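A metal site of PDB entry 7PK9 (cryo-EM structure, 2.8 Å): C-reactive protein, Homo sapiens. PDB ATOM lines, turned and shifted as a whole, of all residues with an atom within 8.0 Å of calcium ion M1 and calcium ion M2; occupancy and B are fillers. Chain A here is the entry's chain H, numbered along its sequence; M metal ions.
Calcium ion M2 is bound by OE1 of Glu 138 (2.3 Å), OE1 of Gln 150 (2.4 Å) and OE1 of Glu 147 (2.8 Å).
Calcium ion M2 has three donor atoms within binding distance.
Slightly farther from calcium ion M2 lies OD2 of Asp 140 (3.0 Å).
Calcium ion M1 is bound by the side-chain carboxylate (OD2) of Asp 60, the side-chain carboxylate (OE2) of Glu 138, the side-chain carboxylate (OD1) of Asp 140 and the side-chain amide oxygen (OD1) of Asn 61.
Calcium ion M1 has four donor atoms within binding distance.
OD1 of Asp 60 sits close to OE1 of Gln 59 (2.9 Å).
O of Gln 150 is in hydrogen-bond range of N of Ser 50, 2.9 Å away.
The backbone NH (N) of Asn 61 is in hydrogen-bond range of the side-chain amide oxygen (OE1) of Gln 59, 2.9 Å away.
The side-chain amide nitrogen (NE2) of Gln 139 sits close to the backbone carbonyl oxygen (O) of Ser 141.
The side-chain hydroxyl of Ser 53 is in hydrogen-bond range of the side-chain amide oxygen of Gln 139, 3.1 Å away.
Within 4 Å of calcium ion M2: Glu 138, Asp 140, Glu 147 and Gln 150.
O of Gln 139 touches calcium ion M1 (3.7 Å).
Of the 23 residues printed, 5 come within 4 Å of calcium ion M1.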
ATOM      1  N   SER A  50       6.840   8.057  26.509  1.00  0.00           N
ATOM      2  CA  SER A  50       6.776   8.443  25.106  1.00  0.00           C
ATOM      3  C   SER A  50       8.160   8.665  24.520  1.00  0.00           C
ATOM      4  O   SER A  50       8.955   9.468  25.032  1.00  0.00           O
ATOM      5  CB  SER A  50       5.945   9.708  24.955  1.00  0.00           C
ATOM      6  OG  SER A  50       5.915  10.141  23.611  1.00  0.00           O
ATOM      7  N   SER A  53       5.665  11.490  19.914  1.00  0.00           N
ATOM      8  CA  SER A  53       4.235  11.776  19.821  1.00  0.00           C
ATOM      9  C   SER A  53       3.949  12.667  18.625  1.00  0.00           C
ATOM     10  O   SER A  53       4.640  13.660  18.385  1.00  0.00           O
ATOM     11  CB  SER A  53       3.755  12.463  21.096  1.00  0.00           C
ATOM     12  OG  SER A  53       2.365  12.696  21.030  1.00  0.00           O
ATOM     13  N   ALA A  55       0.414  14.261  17.270  1.00  0.00           N
ATOM     14  CA  ALA A  55      -1.014  14.438  17.468  1.00  0.00           C
ATOM     15  C   ALA A  55      -1.580  15.355  16.395  1.00  0.00           C
ATOM     16  O   ALA A  55      -1.000  16.398  16.093  1.00  0.00           O
ATOM     17  CB  ALA A  55      -1.302  15.016  18.852  1.00  0.00           C
ATOM     18  N   GLN A  59      -7.070  13.367  16.779  1.00  0.00           N
ATOM     19  CA  GLN A  59      -6.625  12.146  17.434  1.00  0.00           C
ATOM     20  C   GLN A  59      -5.222  12.353  17.979  1.00  0.00           C
ATOM     21  O   GLN A  59      -4.292  12.636  17.225  1.00  0.00           O
ATOM     22  CB  GLN A  59      -6.656  10.959  16.461  1.00  0.00           C
ATOM     23  CG  GLN A  59      -6.001   9.665  16.953  1.00  0.00           C
ATOM     24  CD  GLN A  59      -6.509   9.214  18.301  1.00  0.00           C
ATOM     25  OE1 GLN A  59      -5.832   9.372  19.316  1.00  0.00           O
ATOM     26  NE2 GLN A  59      -7.698   8.617  18.322  1.00  0.00           N
ATOM     27  N   ASP A  60      -5.068  12.201  19.303  1.00  0.00           N
ATOM     28  CA  ASP A  60      -3.823  12.533  19.966  1.00  0.00           C
ATOM     29  C   ASP A  60      -2.752  11.473  19.805  1.00  0.00           C
ATOM     30  O   ASP A  60      -1.577  11.771  20.065  1.00  0.00           O
ATOM     31  CB  ASP A  60      -4.062  12.763  21.461  1.00  0.00           C
ATOM     32  CG  ASP A  60      -4.343  11.483  22.203  1.00  0.00           C
ATOM     33  OD1 ASP A  60      -5.261  10.750  21.771  1.00  0.00           O
ATOM     34  OD2 ASP A  60      -3.625  11.178  23.176  1.00  0.00           O
ATOM     35  N   ASN A  61      -3.101  10.255  19.387  1.00  0.00           N
ATOM     36  CA  ASN A  61      -2.097   9.234  19.151  1.00  0.00           C
ATOM     37  C   ASN A  61      -2.023   8.902  17.669  1.00  0.00           C
ATOM     38  O   ASN A  61      -2.069   7.742  17.282  1.00  0.00           O
ATOM     39  CB  ASN A  61      -2.423   7.965  19.948  1.00  0.00           C
ATOM     40  CG  ASN A  61      -2.329   8.192  21.434  1.00  0.00           C
ATOM     41  OD1 ASN A  61      -1.826   9.206  21.887  1.00  0.00           O
ATOM     42  ND2 ASN A  61      -2.792   7.214  22.204  1.00  0.00           N
ATOM     43  N   GLU A  62      -1.932   9.936  16.839  1.00  0.00           N
ATOM     44  CA  GLU A  62      -1.873   9.725  15.396  1.00  0.00           C
ATOM     45  C   GLU A  62      -0.633   8.954  14.988  1.00  0.00           C
ATOM     46  O   GLU A  62      -0.695   8.051  14.147  1.00  0.00           O
ATOM     47  CB  GLU A  62      -1.938  11.053  14.665  1.00  0.00           C
ATOM     48  CG  GLU A  62      -2.330  10.904  13.213  1.00  0.00           C
ATOM     49  CD  GLU A  62      -3.823  10.905  13.015  1.00  0.00           C
ATOM     50  OE1 GLU A  62      -4.333  10.059  12.248  1.00  0.00           O
ATOM     51  OE2 GLU A  62      -4.504  11.743  13.636  1.00  0.00           O
ATOM     52  N   LEU A  64       2.225   7.332  17.757  1.00  0.00           N
ATOM     53  CA  LEU A  64       2.883   7.227  19.054  1.00  0.00           C
ATOM     54  C   LEU A  64       3.857   6.062  19.013  1.00  0.00           C
ATOM     55  O   LEU A  64       3.466   4.919  18.754  1.00  0.00           O
ATOM     56  CB  LEU A  64       1.883   7.043  20.195  1.00  0.00           C
ATOM     57  CG  LEU A  64       2.391   7.339  21.605  1.00  0.00           C
ATOM     58  CD1 LEU A  64       2.851   8.767  21.790  1.00  0.00           C
ATOM     59  CD2 LEU A  64       1.303   7.004  22.588  1.00  0.00           C
ATOM     60  N   PHE A  66       5.844   4.340  21.788  1.00  0.00           N
ATOM     61  CA  PHE A  66       5.774   4.314  23.249  1.00  0.00           C
ATOM     62  C   PHE A  66       6.443   3.043  23.760  1.00  0.00           C
ATOM     63  O   PHE A  66       6.153   1.946  23.289  1.00  0.00           O
ATOM     64  CB  PHE A  66       4.314   4.358  23.698  1.00  0.00           C
ATOM     65  CG  PHE A  66       4.122   4.773  25.128  1.00  0.00           C
ATOM     66  CD1 PHE A  66       3.909   6.089  25.470  1.00  0.00           C
ATOM     67  CD2 PHE A  66       4.117   3.824  26.135  1.00  0.00           C
ATOM     68  CE1 PHE A  66       3.722   6.457  26.769  1.00  0.00           C
ATOM     69  CE2 PHE A  66       3.923   4.198  27.437  1.00  0.00           C
ATOM     70  CZ  PHE A  66       3.725   5.507  27.756  1.00  0.00           C
ATOM     71  N   THR A  76       1.588   2.736  17.720  1.00  0.00           N
ATOM     72  CA  THR A  76       0.188   2.975  17.382  1.00  0.00           C
ATOM     73  C   THR A  76       0.082   4.092  16.361  1.00  0.00           C
ATOM     74  O   THR A  76       0.739   5.128  16.470  1.00  0.00           O
ATOM     75  CB  THR A  76      -0.655   3.311  18.613  1.00  0.00           C
ATOM     76  OG1 THR A  76      -2.018   3.505  18.209  1.00  0.00           O
ATOM     77  CG2 THR A  76      -0.160   4.535  19.291  1.00  0.00           C
ATOM     78  N   GLN A 137       7.205  14.244  25.735  1.00  0.00           N
ATOM     79  CA  GLN A 137       5.946  14.090  26.433  1.00  0.00           C
ATOM     80  C   GLN A 137       5.091  13.169  25.595  1.00  0.00           C
ATOM     81  O   GLN A 137       5.201  13.158  24.366  1.00  0.00           O
ATOM     82  CB  GLN A 137       5.250  15.441  26.640  1.00  0.00           C
ATOM     83  CG  GLN A 137       6.043  16.452  27.451  1.00  0.00           C
ATOM     84  CD  GLN A 137       6.311  15.984  28.857  1.00  0.00           C
ATOM     85  OE1 GLN A 137       5.625  15.111  29.368  1.00  0.00           O
ATOM     86  NE2 GLN A 137       7.311  16.568  29.497  1.00  0.00           N
ATOM     87  N   GLU A 138       4.231  12.399  26.248  1.00  0.00           N
ATOM     88  CA  GLU A 138       3.092  11.852  25.540  1.00  0.00           C
ATOM     89  C   GLU A 138       2.018  12.915  25.577  1.00  0.00           C
ATOM     90  O   GLU A 138       1.903  13.670  26.552  1.00  0.00           O
ATOM     91  CB  GLU A 138       2.603  10.540  26.148  1.00  0.00           C
ATOM     92  CG  GLU A 138       1.568   9.807  25.280  1.00  0.00           C
ATOM     93  CD  GLU A 138       0.143  10.287  25.461  1.00  0.00           C
ATOM     94  OE1 GLU A 138      -0.199  10.768  26.570  1.00  0.00           O
ATOM     95  OE2 GLU A 138      -0.642  10.196  24.495  1.00  0.00           O
ATOM     96  N   GLN A 139       1.223  12.984  24.525  1.00  0.00           N
ATOM     97  CA  GLN A 139       0.403  14.146  24.257  1.00  0.00           C
ATOM     98  C   GLN A 139      -1.025  13.674  24.098  1.00  0.00           C
ATOM     99  O   GLN A 139      -1.293  12.784  23.285  1.00  0.00           O
ATOM    100  CB  GLN A 139       0.966  14.833  23.008  1.00  0.00           C
ATOM    101  CG  GLN A 139       0.235  15.985  22.425  1.00  0.00           C
ATOM    102  CD  GLN A 139       0.904  16.410  21.138  1.00  0.00           C
ATOM    103  OE1 GLN A 139       1.641  15.638  20.541  1.00  0.00           O
ATOM    104  NE2 GLN A 139       0.711  17.658  20.744  1.00  0.00           N
ATOM    105  N   ASP A 140      -1.935  14.239  24.895  1.00  0.00           N
ATOM    106  CA  ASP A 140      -3.326  13.827  24.916  1.00  0.00           C
ATOM    107  C   ASP A 140      -4.267  14.921  24.442  1.00  0.00           C
ATOM    108  O   ASP A 140      -5.476  14.678  24.334  1.00  0.00           O
ATOM    109  CB  ASP A 140      -3.724  13.387  26.324  1.00  0.00           C
ATOM    110  CG  ASP A 140      -3.212  12.000  26.665  1.00  0.00           C
ATOM    111  OD1 ASP A 140      -2.541  11.396  25.804  1.00  0.00           O
ATOM    112  OD2 ASP A 140      -3.464  11.527  27.785  1.00  0.00           O
ATOM    113  N   SER A 141      -3.742  16.108  24.152  1.00  0.00           N
ATOM    114  CA  SER A 141      -4.448  17.136  23.425  1.00  0.00           C
ATOM    115  C   SER A 141      -3.464  17.719  22.433  1.00  0.00           C
ATOM    116  O   SER A 141      -2.259  17.478  22.521  1.00  0.00           O
ATOM    117  CB  SER A 141      -5.018  18.209  24.357  1.00  0.00           C
ATOM    118  OG  SER A 141      -3.978  18.987  24.924  1.00  0.00           O
ATOM    119  N   GLY A 144      -0.801  19.529  24.515  1.00  0.00           N
ATOM    120  CA  GLY A 144      -0.728  19.521  25.966  1.00  0.00           C
ATOM    121  C   GLY A 144      -1.367  18.332  26.629  1.00  0.00           C
ATOM    122  O   GLY A 144      -1.454  17.257  26.047  1.00  0.00           O
ATOM    123  N   ASN A 145      -1.815  18.518  27.869  1.00  0.00           N
ATOM    124  CA  ASN A 145      -2.324  17.432  28.697  1.00  0.00           C
ATOM    125  C   ASN A 145      -1.273  16.329  28.878  1.00  0.00           C
ATOM    126  O   ASN A 145      -1.579  15.143  28.819  1.00  0.00           O
ATOM    127  CB  ASN A 145      -3.616  16.869  28.105  1.00  0.00           C
ATOM    128  CG  ASN A 145      -4.745  17.902  28.097  1.00  0.00           C
ATOM    129  OD1 ASN A 145      -4.582  19.017  27.612  1.00  0.00           O
ATOM    130  ND2 ASN A 145      -5.894  17.501  28.615  1.00  0.00           N
ATOM    131  N   PHE A 146      -0.032  16.738  29.093  1.00  0.00           N
ATOM    132  CA  PHE A 146       1.062  15.812  29.322  1.00  0.00           C
ATOM    133  C   PHE A 146       0.933  15.121  30.682  1.00  0.00           C
ATOM    134  O   PHE A 146       0.301  15.630  31.609  1.00  0.00           O
ATOM    135  CB  PHE A 146       2.408  16.534  29.285  1.00  0.00           C
ATOM    136  CG  PHE A 146       2.574  17.447  28.114  1.00  0.00           C
ATOM    137  CD1 PHE A 146       2.293  17.025  26.841  1.00  0.00           C
ATOM    138  CD2 PHE A 146       3.046  18.728  28.294  1.00  0.00           C
ATOM    139  CE1 PHE A 146       2.447  17.868  25.773  1.00  0.00           C
ATOM    140  CE2 PHE A 146       3.201  19.570  27.227  1.00  0.00           C
ATOM    141  CZ  PHE A 146       2.905  19.142  25.972  1.00  0.00           C
ATOM    142  N   GLU A 147       1.548  13.953  30.782  1.00  0.00           N
ATOM    143  CA  GLU A 147       1.641  13.213  32.041  1.00  0.00           C
ATOM    144  C   GLU A 147       3.105  13.017  32.406  1.00  0.00           C
ATOM    145  O   GLU A 147       3.888  12.516  31.592  1.00  0.00           O
ATOM    146  CB  GLU A 147       0.952  11.857  31.953  1.00  0.00           C
ATOM    147  CG  GLU A 147      -0.553  11.935  31.906  1.00  0.00           C
ATOM    148  CD  GLU A 147      -1.193  10.588  31.655  1.00  0.00           C
ATOM    149  OE1 GLU A 147      -0.456   9.622  31.384  1.00  0.00           O
ATOM    150  OE2 GLU A 147      -2.435  10.497  31.722  1.00  0.00           O
ATOM    151  N   GLY A 148       3.466  13.407  33.619  1.00  0.00           N
ATOM    152  CA  GLY A 148       4.826  13.182  34.075  1.00  0.00           C
ATOM    153  C   GLY A 148       5.201  11.717  34.080  1.00  0.00           C
ATOM    154  O   GLY A 148       6.335  11.356  33.758  1.00  0.00           O
ATOM    155  N   SER A 149       4.266  10.857  34.458  1.00  0.00           N
ATOM    156  CA  SER A 149       4.486   9.417  34.434  1.00  0.00           C
ATOM    157  C   SER A 149       4.767   8.865  33.037  1.00  0.00           C
ATOM    158  O   SER A 149       5.100   7.685  32.922  1.00  0.00           O
ATOM    159  CB  SER A 149       3.262   8.702  35.005  1.00  0.00           C
ATOM    160  OG  SER A 149       2.105   8.990  34.240  1.00  0.00           O
ATOM    161  N   GLN A 150       4.609   9.669  31.996  1.00  0.00           N
ATOM    162  CA  GLN A 150       4.897   9.231  30.637  1.00  0.00           C
ATOM    163  C   GLN A 150       6.000  10.034  29.931  1.00  0.00           C
ATOM    164  O   GLN A 150       6.316   9.712  28.789  1.00  0.00           O
ATOM    165  CB  GLN A 150       3.606   9.323  29.814  1.00  0.00           C
ATOM    166  CG  GLN A 150       2.531   8.401  30.313  1.00  0.00           C
ATOM    167  CD  GLN A 150       1.434   8.198  29.320  1.00  0.00           C
ATOM    168  OE1 GLN A 150       1.134   9.080  28.519  1.00  0.00           O
ATOM    169  NE2 GLN A 150       0.821   7.022  29.346  1.00  0.00           N
ATOM    170  N   SER A 151       6.580  11.032  30.572  1.00  0.00           N
ATOM    171  CA  SER A 151       7.638  11.801  29.927  1.00  0.00           C
ATOM    172  C   SER A 151       8.886  10.959  29.644  1.00  0.00           C
ATOM    173  O   SER A 151       9.170   9.954  30.298  1.00  0.00           O
ATOM    174  CB  SER A 151       8.013  12.991  30.800  1.00  0.00           C
ATOM    175  OG  SER A 151       8.599  12.544  32.005  1.00  0.00           O
HETATM  176 CA    CA M   1      -2.776   9.614  24.462  1.00  0.00          CA
HETATM  177 CA    CA M   2      -0.886  10.334  28.715  1.00  0.00          CA
